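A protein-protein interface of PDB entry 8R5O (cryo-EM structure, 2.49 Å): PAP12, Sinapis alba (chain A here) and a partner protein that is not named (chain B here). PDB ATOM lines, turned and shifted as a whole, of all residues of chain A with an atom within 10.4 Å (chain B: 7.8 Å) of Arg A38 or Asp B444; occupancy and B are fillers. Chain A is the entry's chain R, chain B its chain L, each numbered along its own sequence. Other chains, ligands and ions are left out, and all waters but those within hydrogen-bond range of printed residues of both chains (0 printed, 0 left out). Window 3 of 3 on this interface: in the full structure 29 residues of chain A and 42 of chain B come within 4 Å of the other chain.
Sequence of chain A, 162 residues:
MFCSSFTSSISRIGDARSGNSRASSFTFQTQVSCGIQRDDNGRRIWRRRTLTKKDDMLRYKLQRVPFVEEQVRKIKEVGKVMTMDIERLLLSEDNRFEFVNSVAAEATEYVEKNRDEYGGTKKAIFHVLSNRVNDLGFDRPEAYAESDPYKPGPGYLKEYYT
Printed residues of chain B that touch a printed residue of chain A: Pro B99, Asp B100, Leu B443, Asp B444, Leu B446, Ser B447, Glu B448, Ala B449 and Ala B454.
Hydrophobic or aromatic side chains of chain B that line the printed part of chain A: Pro B99 and Ala B454.
Among the printed residues, 14 pairs touch across the chains.
Among the printed residues, Asp or Glu carboxylates within 4 Å of a Lys or Arg side-chain nitrogen of the other chain: Arg A44 with Asp B100.
The side-chain carboxylate of Asp B444 lies within hydrogen-bond range of the side-chain amide nitrogen of Gln B440, at 3.0 Å.
The backbone carbonyl oxygen (O) of Gln A37 is in hydrogen-bond range of the backbone NH (N) of Ile A45.
The backbone carbonyl oxygen (O) of Asp B444 is in hydrogen-bond range of the guanidinium group (NE) of Arg A38, at 3.3 Å.
The backbone carbonyl oxygen (O) of Ser B447 sits close to the backbone carbonyl oxygen (O) of Ile A36.
The backbone carbonyl oxygen (O) of Leu B446 is in hydrogen-bond range of the guanidinium group (NE) of Arg A38, at 2.9 Å.
The side-chain carboxylate (OD1) of Asp B100 is in salt-bridge range of the guanidinium group (NH1) of Arg A44 (3.1 Å).
The backbone carbonyl oxygen (O) of Leu B443 lies close to the guanidinium group (NH2) of Arg A38.
N of Ile A36 sits at hydrogen-bond distance from O of Ala B449, at 2.8 Å.
The side-chain carboxylate (OE1) of Glu B448 sits at hydrogen-bond distance from the side-chain amide nitrogen (NE2) of Gln A37 (3.3 Å).
The backbone carbonyl oxygen (O) of Ala B449 is in hydrogen-bond range of the backbone NH (N) of Gly A35 (3.1 Å).
Ile A36 touches Glu B448 (O to CA, 3.8 Å).
Ala B454 touches Ile A36 (CB to CD1, 3.6 Å).
Gln A37 touches Ser B447 (CA to O, 3.3 Å).
Ser B447 touches Arg A38.
NH2 of Arg A44 touches O of Pro B99, 3.6 Å away.
Trp A46 touches Pro B99.
Arg A38 touches four residues of chain B.
Of chain A, only Arg A38 (3.3 Å) comes within 4 Å of Asp B444.
Leu B443 touches just one residue of chain A: Arg A38.
No residue of chain A comes within 4 Å of Ser B445.
Of the printed residues of chain A, Ala B449 touches Gly A35 (3.1 Å) and Ile A36 (2.8 Å).
Printed residues of chain A within 4 Å of Pro B99: Arg A44 (3.6 Å) and Trp A46 (3.5 Å).
Lys B458 touches none of the printed residues of chain A.
The nearest residue of chain B that does not touch Arg A38 is Ser B445 (4.8 Å).
The nearest residue of chain A that does not touch Asp B444 is Arg A44 (7.1 Å).
The nearest printed residue of chain B that does not touch Trp A46 is Asp B100 (5.9 Å).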
ATOM      1  N   GLY A  35     -33.947  16.873  12.932  1.00  0.00           N
ATOM      2  CA  GLY A  35     -32.700  16.334  13.440  1.00  0.00           C
ATOM      3  C   GLY A  35     -32.206  17.043  14.683  1.00  0.00           C
ATOM      4  O   GLY A  35     -32.095  16.439  15.749  1.00  0.00           O
ATOM      5  N   ILE A  36     -31.908  18.332  14.548  1.00  0.00           N
ATOM      6  CA  ILE A  36     -31.446  19.130  15.678  1.00  0.00           C
ATOM      7  C   ILE A  36     -32.658  19.646  16.444  1.00  0.00           C
ATOM      8  O   ILE A  36     -33.524  20.322  15.879  1.00  0.00           O
ATOM      9  CB  ILE A  36     -30.551  20.287  15.213  1.00  0.00           C
ATOM     10  CG1 ILE A  36     -29.200  19.748  14.738  1.00  0.00           C
ATOM     11  CG2 ILE A  36     -30.371  21.307  16.327  1.00  0.00           C
ATOM     12  CD1 ILE A  36     -28.129  20.807  14.604  1.00  0.00           C
ATOM     13  N   GLN A  37     -32.721  19.323  17.732  1.00  0.00           N
ATOM     14  CA  GLN A  37     -33.808  19.746  18.602  1.00  0.00           C
ATOM     15  C   GLN A  37     -33.216  20.243  19.911  1.00  0.00           C
ATOM     16  O   GLN A  37     -32.390  19.558  20.520  1.00  0.00           O
ATOM     17  CB  GLN A  37     -34.787  18.594  18.862  1.00  0.00           C
ATOM     18  CG  GLN A  37     -36.256  18.990  18.844  1.00  0.00           C
ATOM     19  CD  GLN A  37     -36.670  19.803  20.056  1.00  0.00           C
ATOM     20  OE1 GLN A  37     -35.941  19.890  21.042  1.00  0.00           O
ATOM     21  NE2 GLN A  37     -37.853  20.402  19.986  1.00  0.00           N
ATOM     22  N   ARG A  38     -33.635  21.431  20.338  1.00  0.00           N
ATOM     23  CA  ARG A  38     -33.195  21.979  21.615  1.00  0.00           C
ATOM     24  C   ARG A  38     -34.391  22.240  22.522  1.00  0.00           C
ATOM     25  O   ARG A  38     -35.486  22.541  22.050  1.00  0.00           O
ATOM     26  CB  ARG A  38     -32.397  23.270  21.411  1.00  0.00           C
ATOM     27  CG  ARG A  38     -31.176  23.113  20.523  1.00  0.00           C
ATOM     28  CD  ARG A  38     -30.414  24.420  20.389  1.00  0.00           C
ATOM     29  NE  ARG A  38     -29.680  24.489  19.132  1.00  0.00           N
ATOM     30  CZ  ARG A  38     -28.373  24.300  19.010  1.00  0.00           C
ATOM     31  NH1 ARG A  38     -27.608  24.059  20.061  1.00  0.00           N
ATOM     32  NH2 ARG A  38     -27.819  24.361  17.802  1.00  0.00           N
ATOM     33  N   ARG A  44     -29.610  20.850  23.727  1.00  0.00           N
ATOM     34  CA  ARG A  44     -29.987  19.942  22.649  1.00  0.00           C
ATOM     35  C   ARG A  44     -30.476  18.608  23.195  1.00  0.00           C
ATOM     36  O   ARG A  44     -29.878  18.050  24.113  1.00  0.00           O
ATOM     37  CB  ARG A  44     -28.810  19.708  21.700  1.00  0.00           C
ATOM     38  CG  ARG A  44     -28.326  20.954  20.988  1.00  0.00           C
ATOM     39  CD  ARG A  44     -27.346  20.602  19.888  1.00  0.00           C
ATOM     40  NE  ARG A  44     -27.856  19.531  19.042  1.00  0.00           N
ATOM     41  CZ  ARG A  44     -27.297  19.144  17.904  1.00  0.00           C
ATOM     42  NH1 ARG A  44     -26.213  19.735  17.431  1.00  0.00           N
ATOM     43  NH2 ARG A  44     -27.840  18.139  17.225  1.00  0.00           N
ATOM     44  N   ILE A  45     -31.565  18.099  22.626  1.00  0.00           N
ATOM     45  CA  ILE A  45     -32.096  16.788  22.972  1.00  0.00           C
ATOM     46  C   ILE A  45     -32.008  15.898  21.742  1.00  0.00           C
ATOM     47  O   ILE A  45     -32.223  16.355  20.614  1.00  0.00           O
ATOM     48  CB  ILE A  45     -33.542  16.861  23.508  1.00  0.00           C
ATOM     49  CG1 ILE A  45     -34.517  17.309  22.420  1.00  0.00           C
ATOM     50  CG2 ILE A  45     -33.614  17.799  24.701  1.00  0.00           C
ATOM     51  CD1 ILE A  45     -35.968  17.193  22.829  1.00  0.00           C
ATOM     52  N   TRP A  46     -31.665  14.633  21.959  1.00  0.00           N
ATOM     53  CA  TRP A  46     -31.374  13.734  20.856  1.00  0.00           C
ATOM     54  C   TRP A  46     -31.775  12.319  21.236  1.00  0.00           C
ATOM     55  O   TRP A  46     -31.892  11.977  22.416  1.00  0.00           O
ATOM     56  CB  TRP A  46     -29.892  13.798  20.466  1.00  0.00           C
ATOM     57  CG  TRP A  46     -28.959  13.836  21.640  1.00  0.00           C
ATOM     58  CD1 TRP A  46     -28.712  14.901  22.459  1.00  0.00           C
ATOM     59  CD2 TRP A  46     -28.139  12.766  22.117  1.00  0.00           C
ATOM     60  NE1 TRP A  46     -27.795  14.556  23.420  1.00  0.00           N
ATOM     61  CE2 TRP A  46     -27.426  13.250  23.231  1.00  0.00           C
ATOM     62  CE3 TRP A  46     -27.939  11.444  21.712  1.00  0.00           C
ATOM     63  CZ2 TRP A  46     -26.531  12.460  23.944  1.00  0.00           C
ATOM     64  CZ3 TRP A  46     -27.054  10.664  22.420  1.00  0.00           C
ATOM     65  CH2 TRP A  46     -26.359  11.172  23.523  1.00  0.00           C
ATOM     66  N   ARG A  47     -31.981  11.498  20.213  1.00  0.00           N
ATOM     67  CA  ARG A  47     -32.456  10.133  20.385  1.00  0.00           C
ATOM     68  C   ARG A  47     -31.263   9.205  20.569  1.00  0.00           C
ATOM     69  O   ARG A  47     -30.444   9.049  19.657  1.00  0.00           O
ATOM     70  CB  ARG A  47     -33.298   9.715  19.179  1.00  0.00           C
ATOM     71  CG  ARG A  47     -34.128   8.461  19.384  1.00  0.00           C
ATOM     72  CD  ARG A  47     -33.411   7.229  18.879  1.00  0.00           C
ATOM     73  NE  ARG A  47     -33.014   7.364  17.483  1.00  0.00           N
ATOM     74  CZ  ARG A  47     -32.443   6.400  16.775  1.00  0.00           C
ATOM     75  NH1 ARG A  47     -32.195   5.213  17.300  1.00  0.00           N
ATOM     76  NH2 ARG A  47     -32.114   6.634  15.507  1.00  0.00           N
ATOM     77  N   PRO B  99     -25.191  14.425  20.617  1.00  0.00           N
ATOM     78  CA  PRO B  99     -26.227  14.939  19.708  1.00  0.00           C
ATOM     79  C   PRO B  99     -25.835  14.869  18.243  1.00  0.00           C
ATOM     80  O   PRO B  99     -26.713  14.710  17.385  1.00  0.00           O
ATOM     81  CB  PRO B  99     -26.418  16.389  20.179  1.00  0.00           C
ATOM     82  CG  PRO B  99     -25.178  16.718  20.947  1.00  0.00           C
ATOM     83  CD  PRO B  99     -24.752  15.438  21.589  1.00  0.00           C
ATOM     84  N   ASP B 100     -24.548  14.980  17.924  1.00  0.00           N
ATOM     85  CA  ASP B 100     -24.099  14.907  16.541  1.00  0.00           C
ATOM     86  C   ASP B 100     -23.809  13.486  16.074  1.00  0.00           C
ATOM     87  O   ASP B 100     -23.596  13.280  14.874  1.00  0.00           O
ATOM     88  CB  ASP B 100     -22.855  15.780  16.343  1.00  0.00           C
ATOM     89  CG  ASP B 100     -23.163  17.260  16.453  1.00  0.00           C
ATOM     90  OD1 ASP B 100     -24.325  17.642  16.204  1.00  0.00           O
ATOM     91  OD2 ASP B 100     -22.247  18.041  16.787  1.00  0.00           O
ATOM     92  N   GLU B 437     -20.239  34.494  11.382  1.00  0.00           N
ATOM     93  CA  GLU B 437     -20.730  34.502  12.755  1.00  0.00           C
ATOM     94  C   GLU B 437     -22.251  34.570  12.814  1.00  0.00           C
ATOM     95  O   GLU B 437     -22.849  34.083  13.779  1.00  0.00           O
ATOM     96  CB  GLU B 437     -20.107  35.661  13.541  1.00  0.00           C
ATOM     97  CG  GLU B 437     -20.761  37.017  13.329  1.00  0.00           C
ATOM     98  CD  GLU B 437     -20.440  37.627  11.981  1.00  0.00           C
ATOM     99  OE1 GLU B 437     -19.534  37.117  11.288  1.00  0.00           O
ATOM    100  OE2 GLU B 437     -21.098  38.623  11.612  1.00  0.00           O
ATOM    101  N   GLN B 438     -22.890  35.162  11.803  1.00  0.00           N
ATOM    102  CA  GLN B 438     -24.346  35.124  11.731  1.00  0.00           C
ATOM    103  C   GLN B 438     -24.845  33.708  11.471  1.00  0.00           C
ATOM    104  O   GLN B 438     -25.881  33.300  12.008  1.00  0.00           O
ATOM    105  CB  GLN B 438     -24.847  36.082  10.652  1.00  0.00           C
ATOM    106  CG  GLN B 438     -24.639  37.548  10.988  1.00  0.00           C
ATOM    107  CD  GLN B 438     -25.079  38.468   9.870  1.00  0.00           C
ATOM    108  OE1 GLN B 438     -24.805  39.668   9.892  1.00  0.00           O
ATOM    109  NE2 GLN B 438     -25.769  37.911   8.883  1.00  0.00           N
ATOM    110  N   ASP B 439     -24.131  32.948  10.637  1.00  0.00           N
ATOM    111  CA  ASP B 439     -24.470  31.541  10.452  1.00  0.00           C
ATOM    112  C   ASP B 439     -24.242  30.748  11.733  1.00  0.00           C
ATOM    113  O   ASP B 439     -25.032  29.857  12.064  1.00  0.00           O
ATOM    114  CB  ASP B 439     -23.662  30.949   9.298  1.00  0.00           C
ATOM    115  CG  ASP B 439     -24.164  31.400   7.943  1.00  0.00           C
ATOM    116  OD1 ASP B 439     -25.385  31.623   7.803  1.00  0.00           O
ATOM    117  OD2 ASP B 439     -23.341  31.531   7.015  1.00  0.00           O
ATOM    118  N   GLN B 440     -23.168  31.058  12.462  1.00  0.00           N
ATOM    119  CA  GLN B 440     -22.881  30.346  13.705  1.00  0.00           C
ATOM    120  C   GLN B 440     -23.961  30.592  14.753  1.00  0.00           C
ATOM    121  O   GLN B 440     -24.355  29.667  15.473  1.00  0.00           O
ATOM    122  CB  GLN B 440     -21.508  30.753  14.238  1.00  0.00           C
ATOM    123  CG  GLN B 440     -21.237  30.350  15.681  1.00  0.00           C
ATOM    124  CD  GLN B 440     -21.346  28.854  15.918  1.00  0.00           C
ATOM    125  OE1 GLN B 440     -21.102  28.047  15.021  1.00  0.00           O
ATOM    126  NE2 GLN B 440     -21.719  28.478  17.135  1.00  0.00           N
ATOM    127  N   LYS B 441     -24.455  31.828  14.856  1.00  0.00           N
ATOM    128  CA  LYS B 441     -25.525  32.105  15.805  1.00  0.00           C
ATOM    129  C   LYS B 441     -26.861  31.555  15.324  1.00  0.00           C
ATOM    130  O   LYS B 441     -27.724  31.232  16.146  1.00  0.00           O
ATOM    131  CB  LYS B 441     -25.628  33.611  16.070  1.00  0.00           C
ATOM    132  CG  LYS B 441     -26.235  34.414  14.936  1.00  0.00           C
ATOM    133  CD  LYS B 441     -26.108  35.909  15.177  1.00  0.00           C
ATOM    134  CE  LYS B 441     -24.650  36.338  15.223  1.00  0.00           C
ATOM    135  NZ  LYS B 441     -24.497  37.818  15.268  1.00  0.00           N
ATOM    136  N   LEU B 442     -27.050  31.445  14.007  1.00  0.00           N
ATOM    137  CA  LEU B 442     -28.243  30.788  13.484  1.00  0.00           C
ATOM    138  C   LEU B 442     -28.278  29.320  13.885  1.00  0.00           C
ATOM    139  O   LEU B 442     -29.333  28.794  14.256  1.00  0.00           O
ATOM    140  CB  LEU B 442     -28.298  30.933  11.964  1.00  0.00           C
ATOM    141  CG  LEU B 442     -29.420  30.176  11.250  1.00  0.00           C
ATOM    142  CD1 LEU B 442     -30.780  30.658  11.729  1.00  0.00           C
ATOM    143  CD2 LEU B 442     -29.295  30.318   9.743  1.00  0.00           C
ATOM    144  N   LEU B 443     -27.127  28.644  13.823  1.00  0.00           N
ATOM    145  CA  LEU B 443     -27.055  27.247  14.234  1.00  0.00           C
ATOM    146  C   LEU B 443     -27.354  27.079  15.718  1.00  0.00           C
ATOM    147  O   LEU B 443     -27.938  26.068  16.123  1.00  0.00           O
ATOM    148  CB  LEU B 443     -25.675  26.677  13.904  1.00  0.00           C
ATOM    149  CG  LEU B 443     -25.332  26.535  12.422  1.00  0.00           C
ATOM    150  CD1 LEU B 443     -23.848  26.273  12.241  1.00  0.00           C
ATOM    151  CD2 LEU B 443     -26.155  25.421  11.796  1.00  0.00           C
ATOM    152  N   ASP B 444     -26.960  28.051  16.544  1.00  0.00           N
ATOM    153  CA  ASP B 444     -27.250  27.972  17.971  1.00  0.00           C
ATOM    154  C   ASP B 444     -28.717  28.260  18.265  1.00  0.00           C
ATOM    155  O   ASP B 444     -29.254  27.770  19.265  1.00  0.00           O
ATOM    156  CB  ASP B 444     -26.357  28.939  18.745  1.00  0.00           C
ATOM    157  CG  ASP B 444     -24.881  28.666  18.534  1.00  0.00           C
ATOM    158  OD1 ASP B 444     -24.511  27.484  18.377  1.00  0.00           O
ATOM    159  OD2 ASP B 444     -24.091  29.633  18.526  1.00  0.00           O
ATOM    160  N   SER B 445     -29.376  29.047  17.416  1.00  0.00           N
ATOM    161  CA  SER B 445     -30.771  29.411  17.627  1.00  0.00           C
ATOM    162  C   SER B 445     -31.750  28.372  17.095  1.00  0.00           C
ATOM    163  O   SER B 445     -32.957  28.519  17.314  1.00  0.00           O
ATOM    164  CB  SER B 445     -31.064  30.761  16.972  1.00  0.00           C
ATOM    165  OG  SER B 445     -30.910  30.685  15.566  1.00  0.00           O
ATOM    166  N   LEU B 446     -31.268  27.343  16.403  1.00  0.00           N
ATOM    167  CA  LEU B 446     -32.155  26.345  15.825  1.00  0.00           C
ATOM    168  C   LEU B 446     -32.832  25.522  16.914  1.00  0.00           C
ATOM    169  O   LEU B 446     -32.244  25.223  17.957  1.00  0.00           O
ATOM    170  CB  LEU B 446     -31.380  25.421  14.885  1.00  0.00           C
ATOM    171  CG  LEU B 446     -30.808  26.045  13.611  1.00  0.00           C
ATOM    172  CD1 LEU B 446     -29.917  25.055  12.881  1.00  0.00           C
ATOM    173  CD2 LEU B 446     -31.928  26.532  12.705  1.00  0.00           C
ATOM    174  N   SER B 447     -34.089  25.159  16.662  1.00  0.00           N
ATOM    175  CA  SER B 447     -34.824  24.277  17.563  1.00  0.00           C
ATOM    176  C   SER B 447     -35.573  23.156  16.863  1.00  0.00           C
ATOM    177  O   SER B 447     -35.846  22.136  17.504  1.00  0.00           O
ATOM    178  CB  SER B 447     -35.819  25.081  18.408  1.00  0.00           C
ATOM    179  OG  SER B 447     -35.159  26.094  19.148  1.00  0.00           O
ATOM    180  N   GLU B 448     -35.918  23.292  15.584  1.00  0.00           N
ATOM    181  CA  GLU B 448     -36.649  22.268  14.846  1.00  0.00           C
ATOM    182  C   GLU B 448     -36.061  22.107  13.453  1.00  0.00           C
ATOM    183  O   GLU B 448     -36.787  21.995  12.460  1.00  0.00           O
ATOM    184  CB  GLU B 448     -38.137  22.605  14.763  1.00  0.00           C
ATOM    185  CG  GLU B 448     -39.047  21.391  14.757  1.00  0.00           C
ATOM    186  CD  GLU B 448     -39.199  20.780  16.135  1.00  0.00           C
ATOM    187  OE1 GLU B 448     -39.156  21.537  17.127  1.00  0.00           O
ATOM    188  OE2 GLU B 448     -39.357  19.545  16.226  1.00  0.00           O
ATOM    189  N   ALA B 449     -34.736  22.094  13.361  1.00  0.00           N
ATOM    190  CA  ALA B 449     -34.040  22.055  12.084  1.00  0.00           C
ATOM    191  C   ALA B 449     -33.658  20.627  11.721  1.00  0.00           C
ATOM    192  O   ALA B 449     -33.206  19.856  12.571  1.00  0.00           O
ATOM    193  CB  ALA B 449     -32.789  22.933  12.120  1.00  0.00           C
ATOM    194  N   ALA B 454     -28.844  21.984   9.035  1.00  0.00           N
ATOM    195  CA  ALA B 454     -27.676  22.413   9.793  1.00  0.00           C
ATOM    196  C   ALA B 454     -26.390  22.079   9.053  1.00  0.00           C
ATOM    197  O   ALA B 454     -25.426  22.852   9.085  1.00  0.00           O
ATOM    198  CB  ALA B 454     -27.681  21.769  11.177  1.00  0.00           C
ATOM    199  N   VAL B 457     -25.900  24.738   6.452  1.00  0.00           N
ATOM    200  CA  VAL B 457     -25.433  25.992   7.034  1.00  0.00           C
ATOM    201  C   VAL B 457     -23.972  25.880   7.449  1.00  0.00           C
ATOM    202  O   VAL B 457     -23.178  26.802   7.226  1.00  0.00           O
ATOM    203  CB  VAL B 457     -26.330  26.406   8.215  1.00  0.00           C
ATOM    204  CG1 VAL B 457     -25.779  27.652   8.888  1.00  0.00           C
ATOM    205  CG2 VAL B 457     -27.754  26.640   7.744  1.00  0.00           C
ATOM    206  N   LYS B 458     -23.592  24.756   8.063  1.00  0.00           N
ATOM    207  CA  LYS B 458     -22.194  24.555   8.434  1.00  0.00           C
ATOM    208  C   LYS B 458     -21.283  24.587   7.216  1.00  0.00           C
ATOM    209  O   LYS B 458     -20.141  25.049   7.309  1.00  0.00           O
ATOM    210  CB  LYS B 458     -22.024  23.226   9.172  1.00  0.00           C
ATOM    211  CG  LYS B 458     -22.625  23.179  10.565  1.00  0.00           C
ATOM    212  CD  LYS B 458     -22.683  21.746  11.074  1.00  0.00           C
ATOM    213  CE  LYS B 458     -23.231  21.671  12.488  1.00  0.00           C
ATOM    214  NZ  LYS B 458     -22.335  22.346  13.466  1.00  0.00           N
